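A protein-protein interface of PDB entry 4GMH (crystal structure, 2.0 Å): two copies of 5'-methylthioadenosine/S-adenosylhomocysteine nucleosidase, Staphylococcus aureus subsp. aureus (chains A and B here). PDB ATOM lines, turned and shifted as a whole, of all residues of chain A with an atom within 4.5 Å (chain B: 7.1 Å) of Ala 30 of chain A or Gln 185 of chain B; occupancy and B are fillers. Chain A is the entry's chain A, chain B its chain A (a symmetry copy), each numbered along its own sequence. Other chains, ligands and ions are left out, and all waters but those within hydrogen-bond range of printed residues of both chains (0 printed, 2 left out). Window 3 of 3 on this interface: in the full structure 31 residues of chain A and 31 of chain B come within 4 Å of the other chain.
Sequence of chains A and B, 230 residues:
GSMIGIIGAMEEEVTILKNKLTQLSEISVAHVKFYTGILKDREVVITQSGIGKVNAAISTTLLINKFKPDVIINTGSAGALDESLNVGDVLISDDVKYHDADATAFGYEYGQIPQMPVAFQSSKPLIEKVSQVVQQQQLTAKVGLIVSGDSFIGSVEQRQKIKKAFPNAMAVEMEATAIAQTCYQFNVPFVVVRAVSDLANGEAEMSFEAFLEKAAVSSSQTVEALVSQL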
ATOM      1  N   VAL A  29     -34.949 -24.854   9.575  1.00  0.00           N
ATOM      2  CA  VAL A  29     -33.717 -25.100   8.740  1.00  0.00           C
ATOM      3  C   VAL A  29     -32.457 -24.756   9.609  1.00  0.00           C
ATOM      4  O   VAL A  29     -32.376 -23.640  10.160  1.00  0.00           O
ATOM      5  CB  VAL A  29     -33.708 -24.277   7.411  1.00  0.00           C
ATOM      6  CG1 VAL A  29     -32.377 -24.397   6.660  1.00  0.00           C
ATOM      7  CG2 VAL A  29     -34.886 -24.610   6.475  1.00  0.00           C
ATOM      8  N   ALA A  30     -31.505 -25.701   9.741  1.00  0.00           N
ATOM      9  CA  ALA A  30     -30.396 -25.561  10.727  1.00  0.00           C
ATOM     10  C   ALA A  30     -30.967 -25.178  12.129  1.00  0.00           C
ATOM     11  O   ALA A  30     -31.844 -25.866  12.634  1.00  0.00           O
ATOM     12  CB  ALA A  30     -29.346 -24.558  10.221  1.00  0.00           C
ATOM     13  N   HIS A  31     -30.540 -24.064  12.734  1.00  0.00           N
ATOM     14  CA  HIS A  31     -31.080 -23.635  14.065  1.00  0.00           C
ATOM     15  C   HIS A  31     -32.265 -22.664  13.958  1.00  0.00           C
ATOM     16  O   HIS A  31     -32.844 -22.240  15.002  1.00  0.00           O
ATOM     17  CB  HIS A  31     -29.970 -22.921  14.907  1.00  0.00           C
ATOM     18  CG  HIS A  31     -29.659 -21.499  14.458  1.00  0.00           C
ATOM     19  ND1 HIS A  31     -28.899 -21.216  13.335  1.00  0.00           N
ATOM     20  CD2 HIS A  31     -29.994 -20.284  14.997  1.00  0.00           C
ATOM     21  CE1 HIS A  31     -28.783 -19.892  13.201  1.00  0.00           C
ATOM     22  NE2 HIS A  31     -29.462 -19.307  14.182  1.00  0.00           N
ATOM     23  N   VAL A  32     -32.607 -22.260  12.729  1.00  0.00           N
ATOM     24  CA  VAL A  32     -33.512 -21.107  12.515  1.00  0.00           C
ATOM     25  C   VAL A  32     -34.990 -21.583  12.490  1.00  0.00           C
ATOM     26  O   VAL A  32     -35.267 -22.619  11.845  1.00  0.00           O
ATOM     27  CB  VAL A  32     -33.111 -20.333  11.212  1.00  0.00           C
ATOM     28  CG1 VAL A  32     -33.889 -19.047  11.064  1.00  0.00           C
ATOM     29  CG2 VAL A  32     -31.599 -20.049  11.167  1.00  0.00           C
ATOM     30  N   ASN A  55     -25.069 -15.383  13.943  1.00  0.00           N
ATOM     31  CA  ASN A  55     -26.452 -15.979  13.945  1.00  0.00           C
ATOM     32  C   ASN A  55     -27.450 -15.111  13.139  1.00  0.00           C
ATOM     33  O   ASN A  55     -28.293 -15.682  12.363  1.00  0.00           O
ATOM     34  CB  ASN A  55     -26.977 -16.152  15.367  1.00  0.00           C
ATOM     35  CG  ASN A  55     -26.511 -17.490  16.037  1.00  0.00           C
ATOM     36  OD1 ASN A  55     -26.155 -18.454  15.325  1.00  0.00           O
ATOM     37  ND2 ASN A  55     -26.351 -17.491  17.406  1.00  0.00           N
ATOM     38  N   ILE A  58     -26.454 -15.536   9.082  1.00  0.00           N
ATOM     39  CA  ILE A  58     -27.076 -16.826   8.593  1.00  0.00           C
ATOM     40  C   ILE A  58     -28.633 -16.773   8.387  1.00  0.00           C
ATOM     41  O   ILE A  58     -29.139 -17.170   7.282  1.00  0.00           O
ATOM     42  CB  ILE A  58     -26.664 -18.073   9.495  1.00  0.00           C
ATOM     43  CG1 ILE A  58     -25.140 -18.332   9.579  1.00  0.00           C
ATOM     44  CG2 ILE A  58     -27.375 -19.332   8.983  1.00  0.00           C
ATOM     45  CD1 ILE A  58     -24.729 -19.144  10.833  1.00  0.00           C
ATOM     46  N   MET B 116     -24.567 -20.945  22.806  1.00  0.00           N
ATOM     47  CA  MET B 116     -23.709 -21.770  21.938  1.00  0.00           C
ATOM     48  C   MET B 116     -22.595 -22.435  22.811  1.00  0.00           C
ATOM     49  O   MET B 116     -22.422 -22.039  23.919  1.00  0.00           O
ATOM     50  CB  MET B 116     -22.964 -20.865  20.870  1.00  0.00           C
ATOM     51  CG  MET B 116     -23.854 -19.891  20.071  1.00  0.00           C
ATOM     52  SD  MET B 116     -25.104 -20.774  19.068  1.00  0.00           S
ATOM     53  CE  MET B 116     -23.978 -21.755  17.950  1.00  0.00           C
ATOM     54  N   PHE B 120     -15.513 -24.405  19.192  1.00  0.00           N
ATOM     55  CA  PHE B 120     -15.860 -25.335  18.069  1.00  0.00           C
ATOM     56  C   PHE B 120     -14.638 -26.282  17.699  1.00  0.00           C
ATOM     57  O   PHE B 120     -13.499 -25.812  17.602  1.00  0.00           O
ATOM     58  CB  PHE B 120     -16.334 -24.469  16.829  1.00  0.00           C
ATOM     59  CG  PHE B 120     -17.526 -23.505  17.143  1.00  0.00           C
ATOM     60  CD1 PHE B 120     -18.828 -24.000  17.191  1.00  0.00           C
ATOM     61  CD2 PHE B 120     -17.303 -22.121  17.469  1.00  0.00           C
ATOM     62  CE1 PHE B 120     -19.905 -23.176  17.563  1.00  0.00           C
ATOM     63  CE2 PHE B 120     -18.371 -21.281  17.806  1.00  0.00           C
ATOM     64  CZ  PHE B 120     -19.703 -21.821  17.848  1.00  0.00           C
ATOM     65  N   ALA B 180     -16.472 -21.734  11.156  1.00  0.00           N
ATOM     66  CA  ALA B 180     -16.729 -22.919  12.060  1.00  0.00           C
ATOM     67  C   ALA B 180     -18.111 -22.931  12.711  1.00  0.00           C
ATOM     68  O   ALA B 180     -18.808 -24.064  12.790  1.00  0.00           O
ATOM     69  CB  ALA B 180     -15.586 -23.007  13.143  1.00  0.00           C
ATOM     70  N   GLN B 181     -18.548 -21.722  13.162  1.00  0.00           N
ATOM     71  CA  GLN B 181     -19.955 -21.557  13.702  1.00  0.00           C
ATOM     72  C   GLN B 181     -20.993 -21.929  12.606  1.00  0.00           C
ATOM     73  O   GLN B 181     -21.985 -22.656  12.906  1.00  0.00           O
ATOM     74  CB  GLN B 181     -20.241 -20.138  14.329  1.00  0.00           C
ATOM     75  CG  GLN B 181     -21.670 -19.918  14.968  1.00  0.00           C
ATOM     76  CD  GLN B 181     -21.828 -18.548  15.657  1.00  0.00           C
ATOM     77  OE1 GLN B 181     -20.832 -17.899  15.985  1.00  0.00           O
ATOM     78  NE2 GLN B 181     -23.060 -18.105  15.871  1.00  0.00           N
ATOM     79  N   THR B 182     -20.786 -21.474  11.357  1.00  0.00           N
ATOM     80  CA  THR B 182     -21.737 -21.811  10.283  1.00  0.00           C
ATOM     81  C   THR B 182     -21.805 -23.388   9.982  1.00  0.00           C
ATOM     82  O   THR B 182     -22.934 -23.995   9.898  1.00  0.00           O
ATOM     83  CB  THR B 182     -21.446 -20.951   9.011  1.00  0.00           C
ATOM     84  OG1 THR B 182     -21.325 -19.547   9.383  1.00  0.00           O
ATOM     85  CG2 THR B 182     -22.602 -21.208   7.864  1.00  0.00           C
ATOM     86  N   CYS B 183     -20.638 -24.036   9.918  1.00  0.00           N
ATOM     87  CA  CYS B 183     -20.494 -25.525   9.665  1.00  0.00           C
ATOM     88  C   CYS B 183     -21.119 -26.319  10.809  1.00  0.00           C
ATOM     89  O   CYS B 183     -21.697 -27.418  10.593  1.00  0.00           O
ATOM     90  CB  CYS B 183     -18.977 -25.882   9.448  1.00  0.00           C
ATOM     91  SG  CYS B 183     -18.195 -25.388   7.832  1.00  0.00           S
ATOM     92  N   TYR B 184     -21.020 -25.817  12.043  1.00  0.00           N
ATOM     93  CA  TYR B 184     -21.703 -26.463  13.214  1.00  0.00           C
ATOM     94  C   TYR B 184     -23.262 -26.462  13.059  1.00  0.00           C
ATOM     95  O   TYR B 184     -23.962 -27.525  13.298  1.00  0.00           O
ATOM     96  CB  TYR B 184     -21.309 -25.749  14.488  1.00  0.00           C
ATOM     97  CG  TYR B 184     -22.066 -26.128  15.770  1.00  0.00           C
ATOM     98  CD1 TYR B 184     -21.625 -27.188  16.606  1.00  0.00           C
ATOM     99  CD2 TYR B 184     -23.169 -25.360  16.213  1.00  0.00           C
ATOM    100  CE1 TYR B 184     -22.305 -27.501  17.816  1.00  0.00           C
ATOM    101  CE2 TYR B 184     -23.825 -25.654  17.409  1.00  0.00           C
ATOM    102  CZ  TYR B 184     -23.399 -26.740  18.189  1.00  0.00           C
ATOM    103  OH  TYR B 184     -24.057 -27.008  19.369  1.00  0.00           O
ATOM    104  N   GLN B 185     -23.829 -25.294  12.685  1.00  0.00           N
ATOM    105  CA  GLN B 185     -25.274 -25.179  12.445  1.00  0.00           C
ATOM    106  C   GLN B 185     -25.828 -26.141  11.352  1.00  0.00           C
ATOM    107  O   GLN B 185     -26.954 -26.692  11.537  1.00  0.00           O
ATOM    108  CB  GLN B 185     -25.747 -23.715  12.221  1.00  0.00           C
ATOM    109  CG  GLN B 185     -25.456 -22.754  13.360  1.00  0.00           C
ATOM    110  CD  GLN B 185     -26.295 -22.949  14.663  1.00  0.00           C
ATOM    111  OE1 GLN B 185     -26.715 -24.082  15.026  1.00  0.00           O
ATOM    112  NE2 GLN B 185     -26.533 -21.815  15.390  1.00  0.00           N
ATOM    113  N   PHE B 186     -25.080 -26.399  10.281  1.00  0.00           N
ATOM    114  CA  PHE B 186     -25.515 -27.301   9.227  1.00  0.00           C
ATOM    115  C   PHE B 186     -24.855 -28.751   9.299  1.00  0.00           C
ATOM    116  O   PHE B 186     -25.043 -29.553   8.347  1.00  0.00           O
ATOM    117  CB  PHE B 186     -25.224 -26.732   7.777  1.00  0.00           C
ATOM    118  CG  PHE B 186     -26.025 -25.471   7.416  1.00  0.00           C
ATOM    119  CD1 PHE B 186     -27.335 -25.560   6.920  1.00  0.00           C
ATOM    120  CD2 PHE B 186     -25.476 -24.190   7.620  1.00  0.00           C
ATOM    121  CE1 PHE B 186     -28.089 -24.388   6.621  1.00  0.00           C
ATOM    122  CE2 PHE B 186     -26.217 -23.038   7.315  1.00  0.00           C
ATOM    123  CZ  PHE B 186     -27.517 -23.121   6.857  1.00  0.00           C
ATOM    124  N   ASN B 187     -24.073 -29.070  10.328  1.00  0.00           N
ATOM    125  CA  ASN B 187     -23.312 -30.427  10.389  1.00  0.00           C
ATOM    126  C   ASN B 187     -22.348 -30.809   9.236  1.00  0.00           C
ATOM    127  O   ASN B 187     -22.546 -31.870   8.649  1.00  0.00           O
ATOM    128  CB  ASN B 187     -24.282 -31.609  10.488  1.00  0.00           C
ATOM    129  CG  ASN B 187     -25.186 -31.496  11.670  1.00  0.00           C
ATOM    130  OD1 ASN B 187     -24.749 -31.632  12.807  1.00  0.00           O
ATOM    131  ND2 ASN B 187     -26.479 -31.215  11.417  1.00  0.00           N
ATOM    132  N   VAL B 188     -21.357 -29.976   8.891  1.00  0.00           N
ATOM    133  CA  VAL B 188     -20.400 -30.272   7.807  1.00  0.00           C
ATOM    134  C   VAL B 188     -19.029 -30.274   8.444  1.00  0.00           C
ATOM    135  O   VAL B 188     -18.721 -29.323   9.177  1.00  0.00           O
ATOM    136  CB  VAL B 188     -20.443 -29.139   6.689  1.00  0.00           C
ATOM    137  CG1 VAL B 188     -19.409 -29.381   5.558  1.00  0.00           C
ATOM    138  CG2 VAL B 188     -21.896 -28.973   6.129  1.00  0.00           C
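A ring nitrogen (ND1) of His 31 of chain A sits at hydrogen-bond distance from the side-chain amide nitrogen of Gln 185 of chain B (3.2 Å).
OD1 of Asn 55 of chain A lies within hydrogen-bond range of NE2 of Gln 181 of chain B, 3.2 Å away.
OD1 of Asn 55 of chain A lies within hydrogen-bond range of NE2 of Gln 185 of chain B, 3.4 Å away.
Gln 185 of chain B touches Ala 30 of chain A (O to CB, 3.5 Å).
Phe 186 of chain B touches Ala 30 of chain A (CE1 to CB, 3.8 Å).
Met 116 of chain B touches Asn 55 of chain A.
CD1 of Ile 58 of chain A touches OG1 of Thr 182 of chain B, 3.7 Å away.
Ala 30 of chain A touches two residues of chain B.
Gln 185 of chain B touches just these residues of chain A: Ala 30 (3.5 Å), His 31 (3.2 Å) and Asn 55 (3.4 Å).
Of the printed residues of chain A, Gln 181 of chain B touches Asn 55.
Of the printed residues of chain B, His 31 of chain A touches Gln 185.
Printed residues of chain B within 4 Å of Ile 58 of chain A: Thr 182.
Printed residues of chain A within 4 Å of Phe 186 of chain B: Ala 30 (3.8 Å).
The nearest printed residue of chain A that does not touch Gln 181 of chain B is Ile 58 of chain A (4.9 Å).
Of the 11 printed residues of chain B, 5 touch a printed residue of chain A.
Printed residues of chain B that touch a printed residue of chain A: Met 116, Gln 181, Thr 182, Gln 185 and Phe 186.
Printed residues of chain A that touch a printed residue of chain B: Ala 30, His 31, Asn 55 and Ile 58.
Among the printed residues, no Asp or Glu carboxylate lies within 4 Å of a Lys or Arg side-chain nitrogen of the other chain.
No position is printed for both chains.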
